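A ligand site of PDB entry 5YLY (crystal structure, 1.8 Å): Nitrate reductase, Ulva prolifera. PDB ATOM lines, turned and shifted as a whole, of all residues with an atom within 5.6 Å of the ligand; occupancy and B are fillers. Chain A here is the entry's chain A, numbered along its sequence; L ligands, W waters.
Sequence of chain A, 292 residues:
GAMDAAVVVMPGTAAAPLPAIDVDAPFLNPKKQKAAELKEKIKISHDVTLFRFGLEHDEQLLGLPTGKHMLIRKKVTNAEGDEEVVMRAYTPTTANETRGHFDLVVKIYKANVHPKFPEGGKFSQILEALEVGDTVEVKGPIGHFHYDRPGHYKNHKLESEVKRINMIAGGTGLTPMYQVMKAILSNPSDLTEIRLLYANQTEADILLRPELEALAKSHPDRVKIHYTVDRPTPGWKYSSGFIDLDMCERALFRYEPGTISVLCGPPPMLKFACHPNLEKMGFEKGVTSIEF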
ATOM      1  N   HIS A  69     -16.083 -33.147  -4.039  1.00  0.00           N
ATOM      2  CA  HIS A  69     -15.432 -32.403  -5.134  1.00  0.00           C
ATOM      3  C   HIS A  69     -16.071 -32.802  -6.484  1.00  0.00           C
ATOM      4  O   HIS A  69     -17.061 -33.532  -6.511  1.00  0.00           O
ATOM      5  CB  HIS A  69     -13.909 -32.694  -5.114  1.00  0.00           C
ATOM      6  CG  HIS A  69     -13.541 -34.132  -5.390  1.00  0.00           C
ATOM      7  ND1 HIS A  69     -13.369 -35.049  -4.361  1.00  0.00           N
ATOM      8  CD2 HIS A  69     -13.250 -34.739  -6.568  1.00  0.00           C
ATOM      9  CE1 HIS A  69     -13.020 -36.191  -4.945  1.00  0.00           C
ATOM     10  NE2 HIS A  69     -12.928 -36.048  -6.274  1.00  0.00           N
ATOM     11  N   VAL A  86      -9.065 -35.496 -21.192  1.00  0.00           N
ATOM     12  CA  VAL A  86      -8.208 -35.298 -20.019  1.00  0.00           C
ATOM     13  C   VAL A  86      -9.123 -34.854 -18.898  1.00  0.00           C
ATOM     14  O   VAL A  86      -9.951 -33.960 -19.114  1.00  0.00           O
ATOM     15  CB  VAL A  86      -7.067 -34.250 -20.292  1.00  0.00           C
ATOM     16  CG1 VAL A  86      -6.107 -34.156 -19.100  1.00  0.00           C
ATOM     17  CG2 VAL A  86      -6.302 -34.584 -21.575  1.00  0.00           C
ATOM     18  N   ARG A  88      -9.424 -34.215 -14.381  1.00  0.00           N
ATOM     19  CA  ARG A  88      -8.780 -34.035 -13.073  1.00  0.00           C
ATOM     20  C   ARG A  88      -9.830 -33.643 -12.057  1.00  0.00           C
ATOM     21  O   ARG A  88     -10.850 -33.051 -12.436  1.00  0.00           O
ATOM     22  CB  ARG A  88      -7.655 -32.966 -13.098  1.00  0.00           C
ATOM     23  CG  ARG A  88      -6.473 -33.258 -14.014  1.00  0.00           C
ATOM     24  CD  ARG A  88      -5.598 -34.416 -13.572  1.00  0.00           C
ATOM     25  NE  ARG A  88      -4.420 -34.556 -14.427  1.00  0.00           N
ATOM     26  CZ  ARG A  88      -4.315 -35.364 -15.480  1.00  0.00           C
ATOM     27  NH1 ARG A  88      -5.327 -36.139 -15.844  1.00  0.00           N
ATOM     28  NH2 ARG A  88      -3.192 -35.407 -16.192  1.00  0.00           N
ATOM     29  N   ALA A  89      -9.571 -33.946 -10.781  1.00  0.00           N
ATOM     30  CA  ALA A  89     -10.441 -33.573  -9.666  1.00  0.00           C
ATOM     31  C   ALA A  89     -10.178 -32.118  -9.244  1.00  0.00           C
ATOM     32  O   ALA A  89      -9.029 -31.697  -9.237  1.00  0.00           O
ATOM     33  CB  ALA A  89     -10.162 -34.468  -8.475  1.00  0.00           C
ATOM     34  N   TYR A  90     -11.231 -31.367  -8.886  1.00  0.00           N
ATOM     35  CA  TYR A  90     -11.111 -29.983  -8.374  1.00  0.00           C
ATOM     36  C   TYR A  90     -12.151 -29.755  -7.316  1.00  0.00           C
ATOM     37  O   TYR A  90     -13.299 -30.225  -7.438  1.00  0.00           O
ATOM     38  CB  TYR A  90     -11.241 -28.893  -9.470  1.00  0.00           C
ATOM     39  CG  TYR A  90     -10.096 -28.962 -10.443  1.00  0.00           C
ATOM     40  CD1 TYR A  90      -8.869 -28.380 -10.147  1.00  0.00           C
ATOM     41  CD2 TYR A  90     -10.207 -29.713 -11.612  1.00  0.00           C
ATOM     42  CE1 TYR A  90      -7.767 -28.544 -10.987  1.00  0.00           C
ATOM     43  CE2 TYR A  90      -9.125 -29.827 -12.493  1.00  0.00           C
ATOM     44  CZ  TYR A  90      -7.892 -29.295 -12.153  1.00  0.00           C
ATOM     45  OH  TYR A  90      -6.830 -29.526 -12.988  1.00  0.00           O
ATOM     46  N   THR A  91     -11.768 -29.024  -6.287  1.00  0.00           N
ATOM     47  CA  THR A  91     -12.708 -28.544  -5.283  1.00  0.00           C
ATOM     48  C   THR A  91     -12.809 -27.056  -5.548  1.00  0.00           C
ATOM     49  O   THR A  91     -11.844 -26.309  -5.306  1.00  0.00           O
ATOM     50  CB  THR A  91     -12.312 -28.840  -3.846  1.00  0.00           C
ATOM     51  OG1 THR A  91     -12.184 -30.238  -3.662  1.00  0.00           O
ATOM     52  CG2 THR A  91     -13.370 -28.301  -2.840  1.00  0.00           C
ATOM     53  N   PRO A  92     -13.965 -26.584  -6.013  1.00  0.00           N
ATOM     54  CA  PRO A  92     -14.093 -25.122  -6.269  1.00  0.00           C
ATOM     55  C   PRO A  92     -13.947 -24.324  -4.987  1.00  0.00           C
ATOM     56  O   PRO A  92     -14.137 -24.845  -3.887  1.00  0.00           O
ATOM     57  CB  PRO A  92     -15.556 -24.967  -6.747  1.00  0.00           C
ATOM     58  CG  PRO A  92     -15.952 -26.313  -7.192  1.00  0.00           C
ATOM     59  CD  PRO A  92     -15.200 -27.309  -6.360  1.00  0.00           C
ATOM     60  N   VAL A 105      -9.794 -22.319  -8.339  1.00  0.00           N
ATOM     61  CA  VAL A 105      -8.479 -21.679  -8.203  1.00  0.00           C
ATOM     62  C   VAL A 105      -7.497 -22.775  -8.572  1.00  0.00           C
ATOM     63  O   VAL A 105      -7.483 -23.827  -7.939  1.00  0.00           O
ATOM     64  CB  VAL A 105      -8.289 -21.082  -6.783  1.00  0.00           C
ATOM     65  CG1 VAL A 105      -6.827 -20.708  -6.537  1.00  0.00           C
ATOM     66  CG2 VAL A 105      -9.195 -19.882  -6.611  1.00  0.00           C
ATOM     67  N   VAL A 106      -6.730 -22.569  -9.662  1.00  0.00           N
ATOM     68  CA  VAL A 106      -5.880 -23.599 -10.218  1.00  0.00           C
ATOM     69  C   VAL A 106      -4.420 -23.160 -10.306  1.00  0.00           C
ATOM     70  O   VAL A 106      -4.102 -22.113 -10.874  1.00  0.00           O
ATOM     71  CB  VAL A 106      -6.425 -24.112 -11.612  1.00  0.00           C
ATOM     72  CG1 VAL A 106      -5.544 -25.221 -12.199  1.00  0.00           C
ATOM     73  CG2 VAL A 106      -7.889 -24.580 -11.515  1.00  0.00           C
ATOM     74  N   LYS A 107      -3.533 -23.999  -9.774  1.00  0.00           N
ATOM     75  CA  LYS A 107      -2.088 -23.798  -9.927  1.00  0.00           C
ATOM     76  C   LYS A 107      -1.718 -24.286 -11.345  1.00  0.00           C
ATOM     77  O   LYS A 107      -1.972 -25.449 -11.693  1.00  0.00           O
ATOM     78  CB  LYS A 107      -1.333 -24.626  -8.866  1.00  0.00           C
ATOM     79  CG  LYS A 107       0.204 -24.546  -8.990  1.00  0.00           C
ATOM     80  CD  LYS A 107       0.765 -23.194  -8.588  1.00  0.00           C
ATOM     81  CE  LYS A 107       2.177 -23.344  -8.050  1.00  0.00           C
ATOM     82  NZ  LYS A 107       2.644 -22.086  -7.406  1.00  0.00           N
ATOM     83  N   TYR A 109       0.815 -25.558 -13.968  1.00  0.00           N
ATOM     84  CA  TYR A 109       2.122 -26.212 -14.041  1.00  0.00           C
ATOM     85  C   TYR A 109       2.593 -26.042 -15.453  1.00  0.00           C
ATOM     86  O   TYR A 109       2.232 -26.804 -16.352  1.00  0.00           O
ATOM     87  CB  TYR A 109       2.027 -27.692 -13.630  1.00  0.00           C
ATOM     88  CG  TYR A 109       1.708 -27.895 -12.171  1.00  0.00           C
ATOM     89  CD1 TYR A 109       2.629 -27.542 -11.178  1.00  0.00           C
ATOM     90  CD2 TYR A 109       0.515 -28.482 -11.781  1.00  0.00           C
ATOM     91  CE1 TYR A 109       2.338 -27.752  -9.833  1.00  0.00           C
ATOM     92  CE2 TYR A 109       0.212 -28.684 -10.428  1.00  0.00           C
ATOM     93  CZ  TYR A 109       1.133 -28.329  -9.459  1.00  0.00           C
ATOM     94  OH  TYR A 109       0.836 -28.524  -8.138  1.00  0.00           O
ATOM     95  N   LYS A 110       3.341 -24.953 -15.657  1.00  0.00           N
ATOM     96  CA  LYS A 110       3.803 -24.564 -16.966  1.00  0.00           C
ATOM     97  C   LYS A 110       4.970 -25.391 -17.454  1.00  0.00           C
ATOM     98  O   LYS A 110       5.762 -25.908 -16.657  1.00  0.00           O
ATOM     99  CB  LYS A 110       4.104 -23.057 -17.001  1.00  0.00           C
ATOM    100  CG  LYS A 110       2.853 -22.220 -16.774  1.00  0.00           C
ATOM    101  CD  LYS A 110       3.127 -20.738 -16.722  1.00  0.00           C
ATOM    102  CE  LYS A 110       1.876 -20.009 -16.287  1.00  0.00           C
ATOM    103  NZ  LYS A 110       2.104 -18.561 -16.167  1.00  0.00           N
ATOM    104  N   ALA A 111       5.061 -25.543 -18.775  1.00  0.00           N
ATOM    105  CA  ALA A 111       6.128 -26.270 -19.438  1.00  0.00           C
ATOM    106  C   ALA A 111       7.400 -25.420 -19.434  1.00  0.00           C
ATOM    107  O   ALA A 111       7.322 -24.183 -19.390  1.00  0.00           O
ATOM    108  CB  ALA A 111       5.726 -26.589 -20.874  1.00  0.00           C
ATOM    109  N   VAL A 113       9.750 -24.880 -17.122  1.00  0.00           N
ATOM    110  CA  VAL A 113       9.987 -24.087 -15.911  1.00  0.00           C
ATOM    111  C   VAL A 113      10.792 -24.968 -14.948  1.00  0.00           C
ATOM    112  O   VAL A 113      11.911 -24.612 -14.563  1.00  0.00           O
ATOM    113  CB  VAL A 113       8.677 -23.544 -15.283  1.00  0.00           C
ATOM    114  CG1 VAL A 113       8.950 -22.776 -13.996  1.00  0.00           C
ATOM    115  CG2 VAL A 113       7.917 -22.665 -16.270  1.00  0.00           C
ATOM    116  N   HIS A 114      10.225 -26.136 -14.622  1.00  0.00           N
ATOM    117  CA  HIS A 114      10.788 -27.156 -13.733  1.00  0.00           C
ATOM    118  C   HIS A 114      11.632 -28.136 -14.556  1.00  0.00           C
ATOM    119  O   HIS A 114      11.134 -28.674 -15.553  1.00  0.00           O
ATOM    120  CB  HIS A 114       9.637 -27.890 -13.036  1.00  0.00           C
ATOM    121  CG  HIS A 114      10.000 -28.458 -11.704  1.00  0.00           C
ATOM    122  ND1 HIS A 114      10.787 -29.587 -11.595  1.00  0.00           N
ATOM    123  CD2 HIS A 114       9.681 -28.025 -10.462  1.00  0.00           C
ATOM    124  CE1 HIS A 114      10.916 -29.806 -10.298  1.00  0.00           C
ATOM    125  NE2 HIS A 114      10.267 -28.896  -9.575  1.00  0.00           N
ATOM    126  N   PHE A 117      10.092 -31.694 -14.619  1.00  0.00           N
ATOM    127  CA  PHE A 117       8.839 -31.748 -15.361  1.00  0.00           C
ATOM    128  C   PHE A 117       8.866 -30.745 -16.539  1.00  0.00           C
ATOM    129  O   PHE A 117       8.159 -29.738 -16.473  1.00  0.00           O
ATOM    130  CB  PHE A 117       7.645 -31.472 -14.435  1.00  0.00           C
ATOM    131  CG  PHE A 117       7.598 -32.254 -13.134  1.00  0.00           C
ATOM    132  CD1 PHE A 117       7.056 -33.527 -13.092  1.00  0.00           C
ATOM    133  CD2 PHE A 117       8.072 -31.695 -11.947  1.00  0.00           C
ATOM    134  CE1 PHE A 117       7.001 -34.247 -11.896  1.00  0.00           C
ATOM    135  CE2 PHE A 117       8.009 -32.411 -10.755  1.00  0.00           C
ATOM    136  CZ  PHE A 117       7.476 -33.677 -10.729  1.00  0.00           C
ATOM    137  N   GLU A 119       7.572 -30.864 -19.509  1.00  0.00           N
ATOM    138  CA  GLU A 119       6.293 -30.827 -20.222  1.00  0.00           C
ATOM    139  C   GLU A 119       5.178 -30.106 -19.439  1.00  0.00           C
ATOM    140  O   GLU A 119       4.147 -29.766 -20.003  1.00  0.00           O
ATOM    141  CB  GLU A 119       5.856 -32.227 -20.604  1.00  0.00           C
ATOM    142  CG  GLU A 119       6.245 -32.535 -22.036  1.00  0.00           C
ATOM    143  CD  GLU A 119       5.334 -33.506 -22.745  1.00  0.00           C
ATOM    144  OE1 GLU A 119       5.270 -34.676 -22.316  1.00  0.00           O
ATOM    145  OE2 GLU A 119       4.734 -33.118 -23.779  1.00  0.00           O
ATOM    146  N   GLY A 120       5.408 -29.885 -18.141  1.00  0.00           N
ATOM    147  CA  GLY A 120       4.438 -29.239 -17.257  1.00  0.00           C
ATOM    148  C   GLY A 120       3.286 -30.156 -16.927  1.00  0.00           C
ATOM    149  O   GLY A 120       3.375 -31.364 -17.144  1.00  0.00           O
ATOM    150  N   GLY A 121       2.195 -29.574 -16.431  1.00  0.00           N
ATOM    151  CA  GLY A 121       0.981 -30.297 -16.084  1.00  0.00           C
ATOM    152  C   GLY A 121       0.005 -30.262 -17.234  1.00  0.00           C
ATOM    153  O   GLY A 121      -0.274 -29.182 -17.783  1.00  0.00           O
ATOM    154  N   LYS A 122      -0.511 -31.435 -17.633  1.00  0.00           N
ATOM    155  CA  LYS A 122      -1.408 -31.560 -18.784  1.00  0.00           C
ATOM    156  C   LYS A 122      -2.715 -30.723 -18.686  1.00  0.00           C
ATOM    157  O   LYS A 122      -2.957 -29.873 -19.547  1.00  0.00           O
ATOM    158  CB  LYS A 122      -1.717 -33.040 -19.054  1.00  0.00           C
ATOM    159  CG  LYS A 122      -2.411 -33.298 -20.396  1.00  0.00           C
ATOM    160  CD  LYS A 122      -2.052 -34.651 -21.000  1.00  0.00           C
ATOM    161  CE  LYS A 122      -2.631 -35.848 -20.279  1.00  0.00           C
ATOM    162  NZ  LYS A 122      -2.112 -37.135 -20.847  1.00  0.00           N
ATOM    163  N   PHE A 123      -3.561 -30.997 -17.683  1.00  0.00           N
ATOM    164  CA  PHE A 123      -4.856 -30.347 -17.565  1.00  0.00           C
ATOM    165  C   PHE A 123      -4.785 -28.901 -17.068  1.00  0.00           C
ATOM    166  O   PHE A 123      -5.585 -28.078 -17.549  1.00  0.00           O
ATOM    167  CB  PHE A 123      -5.801 -31.174 -16.709  1.00  0.00           C
ATOM    168  CG  PHE A 123      -7.256 -30.862 -17.000  1.00  0.00           C
ATOM    169  CD1 PHE A 123      -7.809 -31.130 -18.252  1.00  0.00           C
ATOM    170  CD2 PHE A 123      -8.044 -30.233 -16.042  1.00  0.00           C
ATOM    171  CE1 PHE A 123      -9.132 -30.802 -18.536  1.00  0.00           C
ATOM    172  CE2 PHE A 123      -9.385 -29.934 -16.313  1.00  0.00           C
ATOM    173  CZ  PHE A 123      -9.924 -30.238 -17.547  1.00  0.00           C
ATOM    174  N   SER A 124      -3.854 -28.553 -16.149  1.00  0.00           N
ATOM    175  CA  SER A 124      -3.759 -27.136 -15.728  1.00  0.00           C
ATOM    176  C   SER A 124      -3.382 -26.222 -16.923  1.00  0.00           C
ATOM    177  O   SER A 124      -3.910 -25.115 -17.026  1.00  0.00           O
ATOM    178  CB  SER A 124      -2.832 -26.945 -14.536  1.00  0.00           C
ATOM    179  OG  SER A 124      -1.517 -27.402 -14.832  1.00  0.00           O
ATOM    180  N   GLN A 125      -2.549 -26.713 -17.886  1.00  0.00           N
ATOM    181  CA  GLN A 125      -2.218 -25.920 -19.082  1.00  0.00           C
ATOM    182  C   GLN A 125      -3.435 -25.901 -20.037  1.00  0.00           C
ATOM    183  O   GLN A 125      -3.684 -24.887 -20.677  1.00  0.00           O
ATOM    184  CB  GLN A 125      -0.951 -26.425 -19.786  1.00  0.00           C
ATOM    185  CG  GLN A 125       0.293 -26.251 -18.950  1.00  0.00           C
ATOM    186  CD  GLN A 125       1.496 -26.867 -19.610  1.00  0.00           C
ATOM    187  OE1 GLN A 125       2.247 -26.191 -20.306  1.00  0.00           O
ATOM    188  NE2 GLN A 125       1.742 -28.153 -19.382  1.00  0.00           N
ATOM    189  N   THR A 172      -1.863 -28.146  -3.736  1.00  0.00           N
ATOM    190  CA  THR A 172      -3.252 -28.026  -4.248  1.00  0.00           C
ATOM    191  C   THR A 172      -4.272 -28.760  -3.357  1.00  0.00           C
ATOM    192  O   THR A 172      -5.481 -28.539  -3.500  1.00  0.00           O
ATOM    193  CB  THR A 172      -3.340 -28.471  -5.731  1.00  0.00           C
ATOM    194  OG1 THR A 172      -2.951 -29.824  -5.858  1.00  0.00           O
ATOM    195  CG2 THR A 172      -2.518 -27.590  -6.655  1.00  0.00           C
ATOM    196  N   THR A 175      -7.649 -26.725  -1.366  1.00  0.00           N
ATOM    197  CA  THR A 175      -9.074 -26.344  -1.640  1.00  0.00           C
ATOM    198  C   THR A 175     -10.098 -27.297  -0.992  1.00  0.00           C
ATOM    199  O   THR A 175     -11.080 -26.740  -0.475  1.00  0.00           O
ATOM    200  CB  THR A 175      -9.326 -26.091  -3.093  1.00  0.00           C
ATOM    201  OG1 THR A 175      -9.041 -27.271  -3.818  1.00  0.00           O
ATOM    202  CG2 THR A 175      -8.482 -24.909  -3.618  1.00  0.00           C
ATOM    203  N   PRO A 176      -9.888 -28.626  -0.824  1.00  0.00           N
ATOM    204  CA  PRO A 176     -10.876 -29.407  -0.039  1.00  0.00           C
ATOM    205  C   PRO A 176     -10.958 -28.890   1.392  1.00  0.00           C
ATOM    206  O   PRO A 176     -12.034 -28.856   1.949  1.00  0.00           O
ATOM    207  CB  PRO A 176     -10.326 -30.838  -0.123  1.00  0.00           C
ATOM    208  CG  PRO A 176      -9.585 -30.873  -1.456  1.00  0.00           C
ATOM    209  CD  PRO A 176      -8.877 -29.527  -1.415  1.00  0.00           C
ATOM    210  N   LEU A 207      -1.160 -21.409  -1.654  1.00  0.00           N
ATOM    211  CA  LEU A 207      -2.377 -20.945  -2.295  1.00  0.00           C
ATOM    212  C   LEU A 207      -3.256 -20.211  -1.281  1.00  0.00           C
ATOM    213  O   LEU A 207      -3.317 -20.598  -0.118  1.00  0.00           O
ATOM    214  CB  LEU A 207      -3.196 -22.127  -2.878  1.00  0.00           C
ATOM    215  CG  LEU A 207      -2.609 -22.855  -4.086  1.00  0.00           C
ATOM    216  CD1 LEU A 207      -3.422 -24.120  -4.406  1.00  0.00           C
ATOM    217  CD2 LEU A 207      -2.579 -21.955  -5.327  1.00  0.00           C
ATOM    218  N   CYS A 264      -5.344 -33.922   2.714  1.00  0.00           N
ATOM    219  CA  CYS A 264      -5.304 -33.862   1.256  1.00  0.00           C
ATOM    220  C   CYS A 264      -3.972 -33.325   0.804  1.00  0.00           C
ATOM    221  O   CYS A 264      -3.572 -32.214   1.172  1.00  0.00           O
ATOM    222  CB  CYS A 264      -6.466 -33.067   0.674  1.00  0.00           C
ATOM    223  SG  CYS A 264      -6.615 -33.233  -1.117  1.00  0.00           S
ATOM    224  N   PHE A 292      -9.085 -37.038   1.739  1.00  0.00           N
ATOM    225  CA  PHE A 292      -9.962 -36.611   0.655  1.00  0.00           C
ATOM    226  C   PHE A 292      -9.445 -37.294  -0.617  1.00  0.00           C
ATOM    227  O   PHE A 292      -8.223 -37.592  -0.686  1.00  0.00           O
ATOM    228  CB  PHE A 292      -9.923 -35.092   0.489  1.00  0.00           C
ATOM    229  CG  PHE A 292     -10.730 -34.321   1.505  1.00  0.00           C
ATOM    230  CD1 PHE A 292     -12.107 -34.277   1.421  1.00  0.00           C
ATOM    231  CD2 PHE A 292     -10.105 -33.541   2.461  1.00  0.00           C
ATOM    232  CE1 PHE A 292     -12.854 -33.516   2.303  1.00  0.00           C
ATOM    233  CE2 PHE A 292     -10.852 -32.772   3.347  1.00  0.00           C
ATOM    234  CZ  PHE A 292     -12.220 -32.764   3.264  1.00  0.00           C
ATOM    235  OXT PHE A 292     -10.241 -37.540  -1.538  1.00  0.00           O
HETATM  236  P1  LIG L   1      -0.277 -33.617 -14.428  1.00  0.00           P
HETATM  237  O1  LIG L   1      -0.079 -33.724 -15.888  1.00  0.00           O
HETATM  238  O2  LIG L   1      -1.285 -34.595 -13.860  1.00  0.00           O
HETATM  239  O3  LIG L   1       1.173 -33.755 -13.714  1.00  0.00           O
HETATM  240  C1  LIG L   1       1.323 -34.571 -12.533  1.00  0.00           C
HETATM  241  C2  LIG L   1       2.093 -33.833 -11.474  1.00  0.00           C
HETATM  242  O4  LIG L   1       3.370 -33.385 -11.982  1.00  0.00           O
HETATM  243  C3  LIG L   1       1.446 -32.555 -10.945  1.00  0.00           C
HETATM  244  O5  LIG L   1       0.399 -32.833 -10.014  1.00  0.00           O
HETATM  245  C4  LIG L   1       2.647 -31.840 -10.312  1.00  0.00           C
HETATM  246  O6  LIG L   1       2.875 -32.259  -8.971  1.00  0.00           O
HETATM  247  C5  LIG L   1       3.807 -32.272 -11.222  1.00  0.00           C
HETATM  248  N1  LIG L   1       4.290 -31.221 -12.133  1.00  0.00           N
HETATM  249  C6  LIG L   1       4.122 -31.181 -13.493  1.00  0.00           C
HETATM  250  N2  LIG L   1       4.622 -30.112 -14.057  1.00  0.00           N
HETATM  251  C7  LIG L   1       5.138 -29.392 -12.996  1.00  0.00           C
HETATM  252  C8  LIG L   1       5.758 -28.121 -12.908  1.00  0.00           C
HETATM  253  N3  LIG L   1       5.797 -27.249 -13.922  1.00  0.00           N
HETATM  254  N4  LIG L   1       6.199 -27.710 -11.700  1.00  0.00           N
HETATM  255  C9  LIG L   1       5.986 -28.494 -10.643  1.00  0.00           C
HETATM  256  N5  LIG L   1       5.365 -29.676 -10.582  1.00  0.00           N
HETATM  257  C10 LIG L   1       4.962 -30.070 -11.809  1.00  0.00           C
HETATM  258  N6  LIG L   1      -5.604 -28.497  -8.146  1.00  0.00           N
HETATM  259  C11 LIG L   1      -5.768 -27.146  -8.221  1.00  0.00           C
HETATM  260  O7  LIG L   1      -4.953 -26.444  -8.835  1.00  0.00           O
HETATM  261  N7  LIG L   1      -6.887 -26.549  -7.606  1.00  0.00           N
HETATM  262  C12 LIG L   1      -7.873 -27.224  -6.885  1.00  0.00           C
HETATM  263  O8  LIG L   1      -8.852 -26.633  -6.467  1.00  0.00           O
HETATM  264  C13 LIG L   1      -7.662 -28.664  -6.784  1.00  0.00           C
HETATM  265  N8  LIG L   1      -8.530 -29.371  -6.091  1.00  0.00           N
HETATM  266  C14 LIG L   1      -8.302 -30.744  -5.971  1.00  0.00           C
HETATM  267  C15 LIG L   1      -9.200 -31.500  -5.206  1.00  0.00           C
HETATM  268  C16 LIG L   1      -9.019 -32.881  -5.043  1.00  0.00           C
HETATM  269  C17 LIG L   1      -9.988 -33.647  -4.187  1.00  0.00           C
HETATM  270  C18 LIG L   1      -7.915 -33.520  -5.663  1.00  0.00           C
HETATM  271  C19 LIG L   1      -7.708 -35.022  -5.556  1.00  0.00           C
HETATM  272  C20 LIG L   1      -7.003 -32.757  -6.402  1.00  0.00           C
HETATM  273  C21 LIG L   1      -7.198 -31.385  -6.567  1.00  0.00           C
HETATM  274  N9  LIG L   1      -6.307 -30.581  -7.352  1.00  0.00           N
HETATM  275  C22 LIG L   1      -6.496 -29.218  -7.464  1.00  0.00           C
HETATM  276  C23 LIG L   1      -5.252 -31.177  -8.179  1.00  0.00           C
HETATM  277  C24 LIG L   1      -5.720 -31.523  -9.595  1.00  0.00           C
HETATM  278  O9  LIG L   1      -6.575 -32.664  -9.580  1.00  0.00           O
HETATM  279  C25 LIG L   1      -4.565 -31.787 -10.554  1.00  0.00           C
HETATM  280  O10 LIG L   1      -3.771 -32.864 -10.074  1.00  0.00           O
HETATM  281  C26 LIG L   1      -3.703 -30.560 -10.860  1.00  0.00           C
HETATM  282  O11 LIG L   1      -4.502 -29.581 -11.510  1.00  0.00           O
HETATM  283  C27 LIG L   1      -2.492 -30.862 -11.723  1.00  0.00           C
HETATM  284  O12 LIG L   1      -2.917 -31.637 -12.868  1.00  0.00           O
HETATM  285  P2  LIG L   1      -2.201 -31.496 -14.299  1.00  0.00           P
HETATM  286  O13 LIG L   1      -2.956 -32.279 -15.304  1.00  0.00           O
HETATM  287  O14 LIG L   1      -1.949 -30.033 -14.611  1.00  0.00           O
HETATM  288  O15 LIG L   1      -0.791 -32.163 -14.008  1.00  0.00           O
HETATM  289  O   HOH W   1      -1.232 -37.385 -14.045  1.00  0.00           O
HETATM  290  O   HOH W   2      -2.262 -34.683 -11.325  1.00  0.00           O
HETATM  291  O   HOH W   3     -10.476 -24.551  -6.873  1.00  0.00           O
HETATM  292  O   HOH W   4      -4.196 -32.003  -4.771  1.00  0.00           O
HETATM  293  O   HOH W   5      -5.619 -35.277  -9.146  1.00  0.00           O
HETATM  294  O   HOH W   6       8.159 -27.011 -16.231  1.00  0.00           O
HETATM  295  O   HOH W   7       0.499 -35.991 -17.403  1.00  0.00           O
HETATM  296  O   HOH W   8       4.250 -35.783 -13.672  1.00  0.00           O
HETATM  297  O   HOH W   9      -3.079 -27.573 -10.408  1.00  0.00           O
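OG of Ser 124 sits at hydrogen-bond distance from O14 of the ligand (2.7 Å).
The guanidinium group of Arg 88 lies within salt-bridge range of an oxygen (O13) of the ligand (2.8 Å).
The backbone NH (N) of Gly 121 sits at hydrogen-bond distance from a nitrogen (N2) of the ligand.
N of Lys 107 sits at hydrogen-bond distance from O7 of the ligand (3.0 Å).
The side-chain hydroxyl (OG1) of Thr 175 is in hydrogen-bond range of an oxygen (O8) of the ligand, 2.7 Å away.
O11 of the ligand sits at hydrogen-bond distance from OH of Tyr 90, 2.8 Å away.
The backbone carbonyl oxygen of Lys 110 sits at hydrogen-bond distance from a nitrogen (N3) of the ligand (3.0 Å).
The backbone NH of Lys 122 is in hydrogen-bond range of an oxygen (O1) of the ligand (2.9 Å).
The backbone NH (N) of Ala 89 lies within hydrogen-bond range of an oxygen (O9) of the ligand (3.5 Å).
N8 of the ligand sits at hydrogen-bond distance from N of Thr 91 (3.3 Å).
A nitrogen (N7) of the ligand is in hydrogen-bond range of the backbone carbonyl oxygen (O) of Val 105, at 2.8 Å.
An oxygen (O9) of the ligand is in hydrogen-bond range of the backbone carbonyl oxygen (O) of Ala 89 (2.7 Å).
The backbone NH of Phe 123 lies within hydrogen-bond range of an oxygen (O13) of the ligand (2.8 Å).
An oxygen (O14) of the ligand sits at hydrogen-bond distance from the backbone NH (N) of Ser 124, 2.9 Å away.
His 69 touches the ligand (ND1 to C17, 3.7 Å).
CA of Val 106 touches O7 of the ligand, at 3.3 Å.
Tyr 109 touches the ligand.
His 114 touches the ligand (CB to N4, 3.7 Å).
CB of Phe 117 touches N2 of the ligand, 3.3 Å away.
Gly 120 touches the ligand.
CB of Thr 172 touches N6 of the ligand (3.3 Å).
CG of Pro 176 touches C15 of the ligand, at 3.8 Å.
Hydrophobic or aromatic side chains within 4 Å of the ligand: His 69, Ala 89, Tyr 90, Val 106, Tyr 109, His 114, Phe 117, Phe 123 and Pro 176.
Within 4 Å of the ligand: His 69, Arg 88, Ala 89, Tyr 90, Thr 91, Val 105, Val 106, Lys 107, Tyr 109, Lys 110, His 114, Phe 117, Gly 120, Gly 121, Lys 122, Phe 123, Ser 124, Thr 172, Thr 175 and Pro 176.
O of Tyr 109 is in hydrogen-bond range of N of Gly 121 (2.8 Å).
O of Tyr 109 lies close to NE2 of Gln 125, 3.4 Å away.
O of Thr 91 is in hydrogen-bond range of OG1 of Thr 175, 3.3 Å away.
The side-chain amide nitrogen (NE2) of Gln 125 sits at hydrogen-bond distance from the backbone carbonyl oxygen (O) of Gly 121 (2.8 Å).
The backbone NH (N) of Tyr 109 is in hydrogen-bond range of the side-chain hydroxyl (OG) of Ser 124 (3.1 Å).
Water W3 lies within hydrogen-bond range of O8 of the ligand (2.7 Å), O of Thr 91 (2.7 Å) and N of Val 105 (2.8 Å).
Water W9 bridges O7 of the ligand (2.7 Å) and O of Lys 107 (2.7 Å).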
